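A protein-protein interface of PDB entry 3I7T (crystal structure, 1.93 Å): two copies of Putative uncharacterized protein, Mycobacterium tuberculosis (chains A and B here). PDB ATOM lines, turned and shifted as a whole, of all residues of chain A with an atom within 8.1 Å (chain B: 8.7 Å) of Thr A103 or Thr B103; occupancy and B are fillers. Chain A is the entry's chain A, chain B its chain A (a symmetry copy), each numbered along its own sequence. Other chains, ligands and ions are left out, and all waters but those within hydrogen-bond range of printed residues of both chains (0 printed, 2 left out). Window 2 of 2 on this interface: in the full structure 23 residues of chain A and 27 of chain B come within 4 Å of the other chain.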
ATOM      1  N   TYR A  72      -9.700 -22.774  18.380  1.00  0.00           N
ATOM      2  CA  TYR A  72      -8.891 -22.017  19.323  1.00  0.00           C
ATOM      3  C   TYR A  72      -7.975 -22.960  20.076  1.00  0.00           C
ATOM      4  O   TYR A  72      -8.439 -23.930  20.674  1.00  0.00           O
ATOM      5  CB  TYR A  72      -9.782 -21.300  20.340  1.00  0.00           C
ATOM      6  CG  TYR A  72     -10.904 -20.506  19.721  1.00  0.00           C
ATOM      7  CD1 TYR A  72     -10.675 -19.238  19.214  1.00  0.00           C
ATOM      8  CD2 TYR A  72     -12.192 -21.022  19.641  1.00  0.00           C
ATOM      9  CE1 TYR A  72     -11.694 -18.493  18.634  1.00  0.00           C
ATOM     10  CE2 TYR A  72     -13.224 -20.284  19.064  1.00  0.00           C
ATOM     11  CZ  TYR A  72     -12.961 -19.016  18.561  1.00  0.00           C
ATOM     12  OH  TYR A  72     -13.973 -18.265  17.981  1.00  0.00           O
ATOM     13  N   VAL A  73      -6.685 -22.648  20.085  1.00  0.00           N
ATOM     14  CA  VAL A  73      -5.721 -23.445  20.819  1.00  0.00           C
ATOM     15  C   VAL A  73      -4.927 -22.581  21.790  1.00  0.00           C
ATOM     16  O   VAL A  73      -4.753 -21.374  21.571  1.00  0.00           O
ATOM     17  CB  VAL A  73      -4.766 -24.198  19.884  1.00  0.00           C
ATOM     18  CG1 VAL A  73      -5.510 -25.282  19.143  1.00  0.00           C
ATOM     19  CG2 VAL A  73      -4.066 -23.219  18.914  1.00  0.00           C
ATOM     20  N   THR A  74      -4.440 -23.185  22.870  1.00  0.00           N
ATOM     21  CA  THR A  74      -3.635 -22.419  23.803  1.00  0.00           C
ATOM     22  C   THR A  74      -2.155 -22.434  23.399  1.00  0.00           C
ATOM     23  O   THR A  74      -1.378 -21.613  23.867  1.00  0.00           O
ATOM     24  CB  THR A  74      -3.836 -22.841  25.292  1.00  0.00           C
ATOM     25  OG1 THR A  74      -3.512 -24.230  25.476  1.00  0.00           O
ATOM     26  CG2 THR A  74      -5.278 -22.568  25.732  1.00  0.00           C
ATOM     27  N   ASP A  75      -1.768 -23.353  22.522  1.00  0.00           N
ATOM     28  CA  ASP A  75      -0.399 -23.370  22.024  1.00  0.00           C
ATOM     29  C   ASP A  75      -0.372 -23.725  20.551  1.00  0.00           C
ATOM     30  O   ASP A  75      -0.406 -24.906  20.190  1.00  0.00           O
ATOM     31  CB  ASP A  75       0.455 -24.363  22.802  1.00  0.00           C
ATOM     32  CG  ASP A  75       1.892 -24.380  22.322  1.00  0.00           C
ATOM     33  OD1 ASP A  75       2.161 -23.784  21.251  1.00  0.00           O
ATOM     34  OD2 ASP A  75       2.749 -24.982  23.012  1.00  0.00           O
ATOM     35  N   ILE A  76      -0.327 -22.703  19.704  1.00  0.00           N
ATOM     36  CA  ILE A  76      -0.445 -22.923  18.265  1.00  0.00           C
ATOM     37  C   ILE A  76       0.804 -23.608  17.686  1.00  0.00           C
ATOM     38  O   ILE A  76       0.804 -24.071  16.540  1.00  0.00           O
ATOM     39  CB  ILE A  76      -0.779 -21.609  17.493  1.00  0.00           C
ATOM     40  CG1 ILE A  76      -1.496 -21.932  16.168  1.00  0.00           C
ATOM     41  CG2 ILE A  76       0.474 -20.753  17.291  1.00  0.00           C
ATOM     42  CD1 ILE A  76      -2.274 -20.791  15.625  1.00  0.00           C
ATOM     43  N   VAL A 100      -6.461 -20.200  15.678  1.00  0.00           N
ATOM     44  CA  VAL A 100      -5.717 -19.117  16.313  1.00  0.00           C
ATOM     45  C   VAL A 100      -5.401 -19.435  17.755  1.00  0.00           C
ATOM     46  O   VAL A 100      -6.117 -20.172  18.426  1.00  0.00           O
ATOM     47  CB  VAL A 100      -6.464 -17.779  16.305  1.00  0.00           C
ATOM     48  CG1 VAL A 100      -6.681 -17.294  14.869  1.00  0.00           C
ATOM     49  CG2 VAL A 100      -7.777 -17.901  17.085  1.00  0.00           C
ATOM     50  N   GLU A 101      -4.324 -18.846  18.239  1.00  0.00           N
ATOM     51  CA  GLU A 101      -3.955 -19.074  19.608  1.00  0.00           C
ATOM     52  C   GLU A 101      -4.626 -18.049  20.513  1.00  0.00           C
ATOM     53  O   GLU A 101      -4.607 -16.848  20.227  1.00  0.00           O
ATOM     54  CB  GLU A 101      -2.451 -18.995  19.741  1.00  0.00           C
ATOM     55  CG  GLU A 101      -1.942 -19.507  21.046  1.00  0.00           C
ATOM     56  CD  GLU A 101      -0.445 -19.505  21.062  1.00  0.00           C
ATOM     57  OE1 GLU A 101       0.161 -20.383  20.413  1.00  0.00           O
ATOM     58  OE2 GLU A 101       0.121 -18.610  21.705  1.00  0.00           O
ATOM     59  N   VAL A 102      -5.217 -18.525  21.607  1.00  0.00           N
ATOM     60  CA  VAL A 102      -5.779 -17.627  22.620  1.00  0.00           C
ATOM     61  C   VAL A 102      -4.998 -17.726  23.938  1.00  0.00           C
ATOM     62  O   VAL A 102      -4.307 -18.716  24.179  1.00  0.00           O
ATOM     63  CB  VAL A 102      -7.283 -17.902  22.853  1.00  0.00           C
ATOM     64  CG1 VAL A 102      -8.076 -17.543  21.603  1.00  0.00           C
ATOM     65  CG2 VAL A 102      -7.512 -19.362  23.239  1.00  0.00           C
ATOM     66  N   THR A 103      -5.118 -16.719  24.796  1.00  0.00           N
ATOM     67  CA  THR A 103      -4.412 -16.781  26.071  1.00  0.00           C
ATOM     68  C   THR A 103      -4.957 -17.882  26.969  1.00  0.00           C
ATOM     69  O   THR A 103      -4.186 -18.578  27.619  1.00  0.00           O
ATOM     70  CB  THR A 103      -4.386 -15.424  26.827  1.00  0.00           C
ATOM     71  OG1 THR A 103      -5.704 -14.859  26.863  1.00  0.00           O
ATOM     72  CG2 THR A 103      -3.442 -14.451  26.144  1.00  0.00           C
ATOM     73  N   ALA A 104      -6.279 -18.051  26.990  1.00  0.00           N
ATOM     74  CA  ALA A 104      -6.913 -19.061  27.845  1.00  0.00           C
ATOM     75  C   ALA A 104      -8.260 -19.537  27.305  1.00  0.00           C
ATOM     76  O   ALA A 104      -8.927 -18.815  26.578  1.00  0.00           O
ATOM     77  CB  ALA A 104      -7.084 -18.515  29.272  1.00  0.00           C
ATOM     78  N   LEU A 105      -8.641 -20.766  27.651  1.00  0.00           N
ATOM     79  CA  LEU A 105     -10.015 -21.226  27.485  1.00  0.00           C
ATOM     80  C   LEU A 105     -10.694 -21.208  28.866  1.00  0.00           C
ATOM     81  O   LEU A 105     -10.083 -20.798  29.850  1.00  0.00           O
ATOM     82  CB  LEU A 105     -10.067 -22.618  26.827  1.00  0.00           C
ATOM     83  CG  LEU A 105      -9.382 -22.684  25.454  1.00  0.00           C
ATOM     84  CD1 LEU A 105      -9.122 -24.116  24.996  1.00  0.00           C
ATOM     85  CD2 LEU A 105     -10.144 -21.892  24.387  1.00  0.00           C
ATOM     86  N   ALA A 107     -11.298 -23.157  31.231  1.00  0.00           N
ATOM     87  CA  ALA A 107     -10.606 -23.819  32.343  1.00  0.00           C
ATOM     88  C   ALA A 107      -9.162 -24.081  31.944  1.00  0.00           C
ATOM     89  O   ALA A 107      -8.874 -24.297  30.763  1.00  0.00           O
ATOM     90  CB  ALA A 107     -11.298 -25.117  32.714  1.00  0.00           C
ATOM     91  N   PRO A 108      -8.247 -24.063  32.925  1.00  0.00           N
ATOM     92  CA  PRO A 108      -6.817 -24.050  32.605  1.00  0.00           C
ATOM     93  C   PRO A 108      -6.287 -25.337  31.958  1.00  0.00           C
ATOM     94  O   PRO A 108      -5.260 -25.293  31.280  1.00  0.00           O
ATOM     95  CB  PRO A 108      -6.129 -23.793  33.955  1.00  0.00           C
ATOM     96  CG  PRO A 108      -7.215 -23.802  35.006  1.00  0.00           C
ATOM     97  CD  PRO A 108      -8.518 -24.155  34.369  1.00  0.00           C
ATOM     98  N   LEU A 110      -7.829 -27.024  29.667  1.00  0.00           N
ATOM     99  CA  LEU A 110      -8.456 -27.138  28.353  1.00  0.00           C
ATOM    100  C   LEU A 110      -7.557 -26.478  27.316  1.00  0.00           C
ATOM    101  O   LEU A 110      -7.177 -25.314  27.468  1.00  0.00           O
ATOM    102  CB  LEU A 110      -9.847 -26.491  28.372  1.00  0.00           C
ATOM    103  CG  LEU A 110     -10.756 -27.163  29.410  1.00  0.00           C
ATOM    104  CD1 LEU A 110     -12.162 -26.575  29.383  1.00  0.00           C
ATOM    105  CD2 LEU A 110     -10.790 -28.671  29.161  1.00  0.00           C
ATOM    106  N   TYR B  72      -8.236 -11.029  13.031  1.00  0.00           N
ATOM    107  CA  TYR B  72      -7.327 -11.288  14.136  1.00  0.00           C
ATOM    108  C   TYR B  72      -6.003 -10.598  13.876  1.00  0.00           C
ATOM    109  O   TYR B  72      -5.392 -10.804  12.829  1.00  0.00           O
ATOM    110  CB  TYR B  72      -7.065 -12.790  14.274  1.00  0.00           C
ATOM    111  CG  TYR B  72      -8.315 -13.632  14.300  1.00  0.00           C
ATOM    112  CD1 TYR B  72      -9.043 -13.778  15.469  1.00  0.00           C
ATOM    113  CD2 TYR B  72      -8.770 -14.280  13.158  1.00  0.00           C
ATOM    114  CE1 TYR B  72     -10.201 -14.543  15.513  1.00  0.00           C
ATOM    115  CE2 TYR B  72      -9.930 -15.053  13.189  1.00  0.00           C
ATOM    116  CZ  TYR B  72     -10.640 -15.177  14.376  1.00  0.00           C
ATOM    117  OH  TYR B  72     -11.797 -15.940  14.428  1.00  0.00           O
ATOM    118  N   VAL B  73      -5.544  -9.818  14.847  1.00  0.00           N
ATOM    119  CA  VAL B  73      -4.262  -9.149  14.734  1.00  0.00           C
ATOM    120  C   VAL B  73      -3.368  -9.483  15.921  1.00  0.00           C
ATOM    121  O   VAL B  73      -3.856  -9.793  17.018  1.00  0.00           O
ATOM    122  CB  VAL B  73      -4.416  -7.628  14.605  1.00  0.00           C
ATOM    123  CG1 VAL B  73      -5.026  -7.279  13.269  1.00  0.00           C
ATOM    124  CG2 VAL B  73      -5.247  -7.061  15.778  1.00  0.00           C
ATOM    125  N   THR B  74      -2.055  -9.427  15.717  1.00  0.00           N
ATOM    126  CA  THR B  74      -1.157  -9.688  16.828  1.00  0.00           C
ATOM    127  C   THR B  74      -0.867  -8.407  17.618  1.00  0.00           C
ATOM    128  O   THR B  74      -0.394  -8.469  18.745  1.00  0.00           O
ATOM    129  CB  THR B  74       0.153 -10.424  16.409  1.00  0.00           C
ATOM    130  OG1 THR B  74       0.879  -9.656  15.434  1.00  0.00           O
ATOM    131  CG2 THR B  74      -0.171 -11.816  15.856  1.00  0.00           C
ATOM    132  N   ASP B  75      -1.162  -7.249  17.038  1.00  0.00           N
ATOM    133  CA  ASP B  75      -0.996  -5.995  17.763  1.00  0.00           C
ATOM    134  C   ASP B  75      -2.126  -5.040  17.438  1.00  0.00           C
ATOM    135  O   ASP B  75      -2.080  -4.336  16.423  1.00  0.00           O
ATOM    136  CB  ASP B  75       0.337  -5.339  17.428  1.00  0.00           C
ATOM    137  CG  ASP B  75       0.546  -4.047  18.190  1.00  0.00           C
ATOM    138  OD1 ASP B  75      -0.435  -3.561  18.804  1.00  0.00           O
ATOM    139  OD2 ASP B  75       1.684  -3.520  18.180  1.00  0.00           O
ATOM    140  N   VAL B 100      -9.955  -8.452  16.882  1.00  0.00           N
ATOM    141  CA  VAL B 100      -9.436  -8.745  18.213  1.00  0.00           C
ATOM    142  C   VAL B 100      -7.977  -9.132  18.166  1.00  0.00           C
ATOM    143  O   VAL B 100      -7.482  -9.664  17.176  1.00  0.00           O
ATOM    144  CB  VAL B 100     -10.177  -9.886  18.918  1.00  0.00           C
ATOM    145  CG1 VAL B 100     -11.640  -9.507  19.161  1.00  0.00           C
ATOM    146  CG2 VAL B 100     -10.035 -11.184  18.116  1.00  0.00           C
ATOM    147  N   GLU B 101      -7.291  -8.882  19.264  1.00  0.00           N
ATOM    148  CA  GLU B 101      -5.899  -9.233  19.317  1.00  0.00           C
ATOM    149  C   GLU B 101      -5.734 -10.658  19.830  1.00  0.00           C
ATOM    150  O   GLU B 101      -6.343 -11.040  20.834  1.00  0.00           O
ATOM    151  CB  GLU B 101      -5.170  -8.259  20.215  1.00  0.00           C
ATOM    152  CG  GLU B 101      -3.686  -8.347  20.107  1.00  0.00           C
ATOM    153  CD  GLU B 101      -3.036  -7.282  20.933  1.00  0.00           C
ATOM    154  OE1 GLU B 101      -3.056  -6.105  20.516  1.00  0.00           O
ATOM    155  OE2 GLU B 101      -2.527  -7.622  22.011  1.00  0.00           O
ATOM    156  N   VAL B 102      -4.908 -11.441  19.140  1.00  0.00           N
ATOM    157  CA  VAL B 102      -4.566 -12.787  19.610  1.00  0.00           C
ATOM    158  C   VAL B 102      -3.083 -12.875  19.996  1.00  0.00           C
ATOM    159  O   VAL B 102      -2.276 -12.055  19.558  1.00  0.00           O
ATOM    160  CB  VAL B 102      -4.922 -13.865  18.559  1.00  0.00           C
ATOM    161  CG1 VAL B 102      -6.434 -13.940  18.385  1.00  0.00           C
ATOM    162  CG2 VAL B 102      -4.238 -13.567  17.227  1.00  0.00           C
ATOM    163  N   THR B 103      -2.718 -13.871  20.796  1.00  0.00           N
ATOM    164  CA  THR B 103      -1.315 -14.007  21.171  1.00  0.00           C
ATOM    165  C   THR B 103      -0.442 -14.370  19.978  1.00  0.00           C
ATOM    166  O   THR B 103       0.656 -13.841  19.841  1.00  0.00           O
ATOM    167  CB  THR B 103      -1.084 -15.003  22.340  1.00  0.00           C
ATOM    168  OG1 THR B 103      -1.789 -16.226  22.087  1.00  0.00           O
ATOM    169  CG2 THR B 103      -1.565 -14.409  23.650  1.00  0.00           C
ATOM    170  N   ALA B 104      -0.934 -15.253  19.110  1.00  0.00           N
ATOM    171  CA  ALA B 104      -0.162 -15.699  17.944  1.00  0.00           C
ATOM    172  C   ALA B 104      -1.047 -16.165  16.789  1.00  0.00           C
ATOM    173  O   ALA B 104      -2.173 -16.590  17.003  1.00  0.00           O
ATOM    174  CB  ALA B 104       0.807 -16.821  18.348  1.00  0.00           C
ATOM    175  N   LEU B 105      -0.532 -16.061  15.565  1.00  0.00           N
ATOM    176  CA  LEU B 105      -1.115 -16.751  14.419  1.00  0.00           C
ATOM    177  C   LEU B 105      -0.236 -17.974  14.102  1.00  0.00           C
ATOM    178  O   LEU B 105       0.733 -18.239  14.809  1.00  0.00           O
ATOM    179  CB  LEU B 105      -1.264 -15.808  13.210  1.00  0.00           C
ATOM    180  CG  LEU B 105      -2.118 -14.564  13.492  1.00  0.00           C
ATOM    181  CD1 LEU B 105      -1.951 -13.485  12.426  1.00  0.00           C
ATOM    182  CD2 LEU B 105      -3.596 -14.910  13.701  1.00  0.00           C
ATOM    183  N   ILE B 106      -0.570 -18.710  13.046  1.00  0.00           N
ATOM    184  CA  ILE B 106       0.082 -19.999  12.752  1.00  0.00           C
ATOM    185  C   ILE B 106       1.609 -19.932  12.593  1.00  0.00           C
ATOM    186  O   ILE B 106       2.309 -20.925  12.811  1.00  0.00           O
ATOM    187  CB  ILE B 106      -0.537 -20.646  11.494  1.00  0.00           C
ATOM    188  CG1 ILE B 106      -0.099 -22.103  11.364  1.00  0.00           C
ATOM    189  CG2 ILE B 106      -0.200 -19.829  10.240  1.00  0.00           C
ATOM    190  CD1 ILE B 106      -0.899 -23.031  12.224  1.00  0.00           C
ATOM    191  N   ALA B 107       2.124 -18.765  12.214  1.00  0.00           N
ATOM    192  CA  ALA B 107       3.568 -18.552  12.076  1.00  0.00           C
ATOM    193  C   ALA B 107       3.925 -17.186  12.639  1.00  0.00           C
ATOM    194  O   ALA B 107       3.112 -16.259  12.583  1.00  0.00           O
ATOM    195  CB  ALA B 107       3.993 -18.653  10.622  1.00  0.00           C
ATOM    196  N   PRO B 108       5.143 -17.053  13.188  1.00  0.00           N
ATOM    197  CA  PRO B 108       5.475 -15.864  13.977  1.00  0.00           C
ATOM    198  C   PRO B 108       5.552 -14.557  13.175  1.00  0.00           C
ATOM    199  O   PRO B 108       5.398 -13.482  13.757  1.00  0.00           O
ATOM    200  CB  PRO B 108       6.836 -16.197  14.610  1.00  0.00           C
ATOM    201  CG  PRO B 108       7.269 -17.526  14.035  1.00  0.00           C
ATOM    202  CD  PRO B 108       6.283 -17.966  13.004  1.00  0.00           C
ATOM    203  N   LEU B 110       3.473 -13.690  10.850  1.00  0.00           N
ATOM    204  CA  LEU B 110       2.125 -13.397  10.371  1.00  0.00           C
ATOM    205  C   LEU B 110       1.421 -12.507  11.386  1.00  0.00           C
ATOM    206  O   LEU B 110       1.350 -12.844  12.571  1.00  0.00           O
ATOM    207  CB  LEU B 110       1.348 -14.701  10.145  1.00  0.00           C
ATOM    208  CG  LEU B 110       2.053 -15.594   9.116  1.00  0.00           C
ATOM    209  CD1 LEU B 110       1.248 -16.857   8.831  1.00  0.00           C
ATOM    210  CD2 LEU B 110       2.295 -14.801   7.832  1.00  0.00           C
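N of Val A102 lies within hydrogen-bond range of O of Val A73 (2.9 Å).
OE1 of Glu A101 is in hydrogen-bond range of N of Ile A76 (2.5 Å).
The backbone carbonyl oxygen (O) of Val B73 sits at hydrogen-bond distance from the backbone NH (N) of Val B102 (2.9 Å).
Glu A101 touches Val B102, but with the chains exchanged Val A102 does not touch Glu B101 (6.8 Å).
Glu A101 touches Thr B103, but with the chains exchanged Thr A103 does not touch Glu B101 (6.9 Å).
Glu A101 touches Ala B104, but with the chains exchanged Ala A104 does not touch Glu B101 (9.3 Å).
Val A102 touches Thr B103, but with the chains exchanged Thr A103 does not touch Val B102 (6.4 Å).
13 positions are printed for both chains.
Of the 7 pairs that touch across the chains among the printed residues, 1 has its exchanged pair printed and touching as well.
Of the 14 printed residues of chain A, 4 touch a printed residue of chain B.
Printed residues of chain A that touch a printed residue of chain B: Ile A76, Glu A101, Val A102 and Thr A103.
Hydrophobic or aromatic side chains of chain A within 4 Å of the printed part of chain B: Ile A76.
Printed residues of chain A within 4 Å of Thr B103: Glu A101, Val A102 and Thr A103.
No residue of chain B comes within 4 Å of Ala A104.
Printed residues of chain B within 4 Å of Glu A101: Val B102 (3.4 Å), Thr B103 (3.1 Å) and Ala B104 (3.4 Å).
Of the printed residues of chain A, Ile B106 touches Ile A76.
Printed residues of chain A within 4 Å of Ala B104: Glu A101 (3.4 Å).
Of the printed residues of chain A, Leu B105 touches Ile A76 (3.5 Å).
Of the printed residues of chain B, Ile A76 touches Leu B105 (3.5 Å) and Ile B106 (3.7 Å).
The nearest printed residue of chain A that does not touch Val B102 is Val A100 (4.4 Å).
The side-chain carboxylate of Glu A101 lies within hydrogen-bond range of the side-chain hydroxyl of Thr B103 (3.1 Å).
The backbone carbonyl oxygen (O) of Ala B104 lies within hydrogen-bond range of the backbone NH (N) of Glu A101 (3.4 Å).
Leu B105 touches Ile A76.
Ile B106 touches Ile A76 (N to CD1, 3.7 Å).
CB of Val B102 touches O of Glu A101 (3.4 Å).
Val A102 touches Thr B103 (C to OG1, 3.997 Å).
Thr A103 touches Thr B103.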
